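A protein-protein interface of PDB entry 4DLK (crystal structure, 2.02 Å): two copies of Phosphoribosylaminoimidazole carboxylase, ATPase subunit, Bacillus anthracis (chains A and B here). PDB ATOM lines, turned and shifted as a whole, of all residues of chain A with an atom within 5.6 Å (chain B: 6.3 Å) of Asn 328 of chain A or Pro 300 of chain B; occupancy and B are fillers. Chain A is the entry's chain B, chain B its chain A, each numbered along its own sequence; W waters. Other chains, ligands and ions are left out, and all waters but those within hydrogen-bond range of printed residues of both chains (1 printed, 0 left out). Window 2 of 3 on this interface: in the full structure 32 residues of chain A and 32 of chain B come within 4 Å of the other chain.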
ATOM      1  N   LEU A 324      34.161 -30.263 -22.767  1.00  0.00           N
ATOM      2  CA  LEU A 324      32.994 -31.070 -22.394  1.00  0.00           C
ATOM      3  C   LEU A 324      31.917 -30.234 -21.706  1.00  0.00           C
ATOM      4  O   LEU A 324      30.728 -30.415 -21.963  1.00  0.00           O
ATOM      5  CB  LEU A 324      33.409 -32.263 -21.518  1.00  0.00           C
ATOM      6  CG  LEU A 324      34.349 -33.279 -22.182  1.00  0.00           C
ATOM      7  CD1 LEU A 324      35.025 -34.193 -21.170  1.00  0.00           C
ATOM      8  CD2 LEU A 324      33.620 -34.095 -23.244  1.00  0.00           C
ATOM      9  N   ARG A 325      32.341 -29.307 -20.852  1.00  0.00           N
ATOM     10  CA  ARG A 325      31.418 -28.402 -20.168  1.00  0.00           C
ATOM     11  C   ARG A 325      30.779 -27.393 -21.134  1.00  0.00           C
ATOM     12  O   ARG A 325      29.620 -27.028 -20.976  1.00  0.00           O
ATOM     13  CB  ARG A 325      32.148 -27.676 -19.035  1.00  0.00           C
ATOM     14  CG  ARG A 325      31.239 -27.042 -17.988  1.00  0.00           C
ATOM     15  CD  ARG A 325      32.022 -26.195 -16.986  1.00  0.00           C
ATOM     16  NE  ARG A 325      32.841 -25.184 -17.656  1.00  0.00           N
ATOM     17  CZ  ARG A 325      34.171 -25.202 -17.719  1.00  0.00           C
ATOM     18  NH1 ARG A 325      34.870 -26.170 -17.128  1.00  0.00           N
ATOM     19  NH2 ARG A 325      34.806 -24.236 -18.370  1.00  0.00           N
ATOM     20  N   GLN A 326      31.538 -26.951 -22.135  1.00  0.00           N
ATOM     21  CA  GLN A 326      31.055 -25.948 -23.091  1.00  0.00           C
ATOM     22  C   GLN A 326      30.544 -26.573 -24.387  1.00  0.00           C
ATOM     23  O   GLN A 326      30.412 -25.888 -25.410  1.00  0.00           O
ATOM     24  CB  GLN A 326      32.164 -24.939 -23.406  1.00  0.00           C
ATOM     25  CG  GLN A 326      32.709 -24.189 -22.195  1.00  0.00           C
ATOM     26  CD  GLN A 326      31.894 -22.967 -21.839  1.00  0.00           C
ATOM     27  OE1 GLN A 326      30.660 -23.015 -21.773  1.00  0.00           O
ATOM     28  NE2 GLN A 326      32.582 -21.857 -21.598  1.00  0.00           N
ATOM     29  N   VAL A 327      30.247 -27.871 -24.334  1.00  0.00           N
ATOM     30  CA  VAL A 327      29.898 -28.643 -25.522  1.00  0.00           C
ATOM     31  C   VAL A 327      28.672 -28.078 -26.249  1.00  0.00           C
ATOM     32  O   VAL A 327      28.604 -28.128 -27.474  1.00  0.00           O
ATOM     33  CB  VAL A 327      29.731 -30.150 -25.196  1.00  0.00           C
ATOM     34  CG1 VAL A 327      28.350 -30.449 -24.619  1.00  0.00           C
ATOM     35  CG2 VAL A 327      30.006 -31.001 -26.427  1.00  0.00           C
ATOM     36  N   ASN A 328      27.727 -27.523 -25.489  1.00  0.00           N
ATOM     37  CA  ASN A 328      26.529 -26.903 -26.054  1.00  0.00           C
ATOM     38  C   ASN A 328      26.807 -25.617 -26.847  1.00  0.00           C
ATOM     39  O   ASN A 328      25.949 -25.139 -27.581  1.00  0.00           O
ATOM     40  CB  ASN A 328      25.457 -26.664 -24.970  1.00  0.00           C
ATOM     41  CG  ASN A 328      25.955 -25.813 -23.802  1.00  0.00           C
ATOM     42  OD1 ASN A 328      27.091 -25.955 -23.323  1.00  0.00           O
ATOM     43  ND2 ASN A 328      25.084 -24.943 -23.313  1.00  0.00           N
ATOM     44  N   ARG A 329      28.005 -25.064 -26.702  1.00  0.00           N
ATOM     45  CA  ARG A 329      28.336 -23.804 -27.376  1.00  0.00           C
ATOM     46  C   ARG A 329      29.114 -23.998 -28.677  1.00  0.00           C
ATOM     47  O   ARG A 329      29.501 -23.019 -29.325  1.00  0.00           O
ATOM     48  CB  ARG A 329      29.084 -22.870 -26.416  1.00  0.00           C
ATOM     49  CG  ARG A 329      28.240 -22.413 -25.234  1.00  0.00           C
ATOM     50  CD  ARG A 329      29.080 -21.649 -24.230  1.00  0.00           C
ATOM     51  NE  ARG A 329      29.410 -20.304 -24.700  1.00  0.00           N
ATOM     52  CZ  ARG A 329      30.547 -19.675 -24.424  1.00  0.00           C
ATOM     53  NH1 ARG A 329      31.481 -20.274 -23.698  1.00  0.00           N
ATOM     54  NH2 ARG A 329      30.763 -18.451 -24.887  1.00  0.00           N
ATOM     55  N   LEU A 330      29.313 -25.259 -29.069  1.00  0.00           N
ATOM     56  CA  LEU A 330      30.168 -25.592 -30.214  1.00  0.00           C
ATOM     57  C   LEU A 330      29.481 -25.588 -31.583  1.00  0.00           C
ATOM     58  O   LEU A 330      29.783 -26.431 -32.436  1.00  0.00           O
ATOM     59  CB  LEU A 330      30.883 -26.932 -29.991  1.00  0.00           C
ATOM     60  CG  LEU A 330      31.913 -27.030 -28.853  1.00  0.00           C
ATOM     61  CD1 LEU A 330      32.477 -28.442 -28.776  1.00  0.00           C
ATOM     62  CD2 LEU A 330      33.032 -26.016 -29.022  1.00  0.00           C
ATOM     63  N   THR A 331      28.573 -24.638 -31.801  1.00  0.00           N
ATOM     64  CA  THR A 331      27.991 -24.415 -33.130  1.00  0.00           C
ATOM     65  C   THR A 331      29.095 -23.967 -34.096  1.00  0.00           C
ATOM     66  O   THR A 331      29.981 -23.206 -33.710  1.00  0.00           O
ATOM     67  CB  THR A 331      26.799 -23.417 -33.091  1.00  0.00           C
ATOM     68  OG1 THR A 331      26.410 -23.062 -34.424  1.00  0.00           O
ATOM     69  CG2 THR A 331      27.144 -22.150 -32.320  1.00  0.00           C
ATOM     70  N   ILE B   4      22.343 -34.406 -22.249  1.00  0.00           N
ATOM     71  CA  ILE B   4      23.453 -34.518 -23.199  1.00  0.00           C
ATOM     72  C   ILE B   4      24.218 -35.826 -22.996  1.00  0.00           C
ATOM     73  O   ILE B   4      24.519 -36.213 -21.867  1.00  0.00           O
ATOM     74  CB  ILE B   4      24.419 -33.315 -23.073  1.00  0.00           C
ATOM     75  CG1 ILE B   4      23.703 -32.007 -23.460  1.00  0.00           C
ATOM     76  CG2 ILE B   4      25.672 -33.518 -23.926  1.00  0.00           C
ATOM     77  CD1 ILE B   4      24.467 -30.746 -23.086  1.00  0.00           C
ATOM     78  N   GLU B 202      16.695 -28.271 -32.032  1.00  0.00           N
ATOM     79  CA  GLU B 202      17.434 -27.637 -33.135  1.00  0.00           C
ATOM     80  C   GLU B 202      17.209 -28.416 -34.429  1.00  0.00           C
ATOM     81  O   GLU B 202      17.187 -29.645 -34.412  1.00  0.00           O
ATOM     82  CB  GLU B 202      18.942 -27.543 -32.849  1.00  0.00           C
ATOM     83  CG  GLU B 202      19.695 -26.734 -33.905  1.00  0.00           C
ATOM     84  CD  GLU B 202      21.193 -26.605 -33.655  1.00  0.00           C
ATOM     85  OE1 GLU B 202      21.815 -25.739 -34.300  1.00  0.00           O
ATOM     86  OE2 GLU B 202      21.756 -27.346 -32.825  1.00  0.00           O
ATOM     87  N   GLN B 291      25.491 -35.827 -38.255  1.00  0.00           N
ATOM     88  CA  GLN B 291      24.299 -35.114 -37.806  1.00  0.00           C
ATOM     89  C   GLN B 291      23.444 -36.000 -36.902  1.00  0.00           C
ATOM     90  O   GLN B 291      22.939 -35.544 -35.881  1.00  0.00           O
ATOM     91  CB  GLN B 291      23.478 -34.621 -38.998  1.00  0.00           C
ATOM     92  CG  GLN B 291      24.130 -33.482 -39.772  1.00  0.00           C
ATOM     93  CD  GLN B 291      24.178 -32.182 -38.983  1.00  0.00           C
ATOM     94  OE1 GLN B 291      24.688 -32.128 -37.855  1.00  0.00           O
ATOM     95  NE2 GLN B 291      23.651 -31.126 -39.575  1.00  0.00           N
ATOM     96  N   ARG B 294      25.001 -36.290 -33.426  1.00  0.00           N
ATOM     97  CA  ARG B 294      24.850 -35.028 -32.710  1.00  0.00           C
ATOM     98  C   ARG B 294      23.425 -34.855 -32.224  1.00  0.00           C
ATOM     99  O   ARG B 294      23.213 -34.440 -31.090  1.00  0.00           O
ATOM    100  CB  ARG B 294      25.259 -33.833 -33.579  1.00  0.00           C
ATOM    101  CG  ARG B 294      26.758 -33.698 -33.790  1.00  0.00           C
ATOM    102  CD  ARG B 294      27.078 -32.640 -34.843  1.00  0.00           C
ATOM    103  NE  ARG B 294      28.508 -32.339 -34.908  1.00  0.00           N
ATOM    104  CZ  ARG B 294      29.419 -33.101 -35.517  1.00  0.00           C
ATOM    105  NH1 ARG B 294      29.059 -34.229 -36.119  1.00  0.00           N
ATOM    106  NH2 ARG B 294      30.702 -32.730 -35.537  1.00  0.00           N
ATOM    107  N   ASN B 298      22.310 -34.863 -28.338  1.00  0.00           N
ATOM    108  CA  ASN B 298      21.941 -33.483 -28.040  1.00  0.00           C
ATOM    109  C   ASN B 298      23.138 -32.538 -28.089  1.00  0.00           C
ATOM    110  O   ASN B 298      23.280 -31.662 -27.237  1.00  0.00           O
ATOM    111  CB  ASN B 298      21.194 -33.364 -26.697  1.00  0.00           C
ATOM    112  CG  ASN B 298      20.289 -32.144 -26.639  1.00  0.00           C
ATOM    113  OD1 ASN B 298      19.969 -31.556 -27.663  1.00  0.00           O
ATOM    114  ND2 ASN B 298      19.858 -31.773 -25.434  1.00  0.00           N
ATOM    115  N   LEU B 299      24.003 -32.737 -29.080  1.00  0.00           N
ATOM    116  CA  LEU B 299      25.078 -31.784 -29.345  1.00  0.00           C
ATOM    117  C   LEU B 299      24.589 -30.741 -30.353  1.00  0.00           C
ATOM    118  O   LEU B 299      23.606 -30.980 -31.066  1.00  0.00           O
ATOM    119  CB  LEU B 299      26.333 -32.488 -29.880  1.00  0.00           C
ATOM    120  CG  LEU B 299      26.908 -33.663 -29.081  1.00  0.00           C
ATOM    121  CD1 LEU B 299      28.134 -34.227 -29.780  1.00  0.00           C
ATOM    122  CD2 LEU B 299      27.233 -33.286 -27.643  1.00  0.00           C
ATOM    123  N   PRO B 300      25.278 -29.585 -30.440  1.00  0.00           N
ATOM    124  CA  PRO B 300      24.873 -28.626 -31.465  1.00  0.00           C
ATOM    125  C   PRO B 300      25.046 -29.266 -32.837  1.00  0.00           C
ATOM    126  O   PRO B 300      26.068 -29.924 -33.090  1.00  0.00           O
ATOM    127  CB  PRO B 300      25.877 -27.480 -31.283  1.00  0.00           C
ATOM    128  CG  PRO B 300      26.331 -27.601 -29.864  1.00  0.00           C
ATOM    129  CD  PRO B 300      26.427 -29.090 -29.663  1.00  0.00           C
ATOM    130  N   LEU B 301      24.051 -29.098 -33.705  1.00  0.00           N
ATOM    131  CA  LEU B 301      24.112 -29.683 -35.038  1.00  0.00           C
ATOM    132  C   LEU B 301      25.126 -28.937 -35.899  1.00  0.00           C
ATOM    133  O   LEU B 301      25.341 -27.741 -35.712  1.00  0.00           O
ATOM    134  CB  LEU B 301      22.727 -29.681 -35.703  1.00  0.00           C
ATOM    135  CG  LEU B 301      21.580 -30.377 -34.949  1.00  0.00           C
ATOM    136  CD1 LEU B 301      20.261 -30.264 -35.713  1.00  0.00           C
ATOM    137  CD2 LEU B 301      21.907 -31.837 -34.655  1.00  0.00           C
ATOM    138  N   GLY B 302      25.755 -29.651 -36.824  1.00  0.00           N
ATOM    139  CA  GLY B 302      26.666 -29.031 -37.787  1.00  0.00           C
ATOM    140  C   GLY B 302      25.874 -28.398 -38.921  1.00  0.00           C
ATOM    141  O   GLY B 302      24.657 -28.549 -38.986  1.00  0.00           O
HETATM  142  O   HOH W   1      24.423 -25.775 -34.400  1.00  0.00           O
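Among the printed residues, merely in contact across the chains: Val 327 of chain A with Pro 300 of chain B, Asn 328 of chain A with Pro 300 of chain B, Val 327 of chain A with Leu 299 of chain B, Leu 330 of chain A with Pro 300 of chain B and Thr 331 of chain A with Pro 300 of chain B.
Of chain B, only Pro 300 (3.4 Å) comes within 4 Å of Asn 328 of chain A. Pro 300 of chain B touches just these residues of chain A: Val 327 (3.2 Å), Asn 328 (3.4 Å), Leu 330 (3.9 Å) and Thr 331 (3.95 Å). Printed residues of chain A within 4 Å of Leu 299 of chain B: Val 327. Printed residues of chain B within 4 Å of Leu 330 of chain A: Pro 300 (3.9 Å). Of the printed residues of chain B, Val 327 of chain A touches Leu 299 (3.8 Å) and Pro 300 (3.2 Å). Of the printed residues of chain B, Thr 331 of chain A touches Pro 300. The nearest residue of chain A that does not touch Pro 300 of chain B is Arg 329 of chain A (4.4 Å). The nearest printed residue of chain B that does not touch Val 327 of chain A is Ile 4 of chain B (4.1 Å).
Water W1 lies within hydrogen-bond range of O of Leu 301 of chain B (2.5 Å), OE1 of Glu 202 of chain B (2.6 Å) and OG1 of Thr 331 of chain A (3.4 Å).
No position is printed for both chains.
The backbone carbonyl oxygen of Arg 294 of chain B is in hydrogen-bond range of the backbone NH of Leu 299 of chain B.
Of the 9 printed residues of chain B, 2 touch a printed residue of chain A. Of the 8 printed residues of chain A, 4 touch a printed residue of chain B. Printed residues of chain A that touch a printed residue of chain B: Val 327, Asn 328, Leu 330 and Thr 331. Among the printed residues, 5 pairs touch across the chains.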
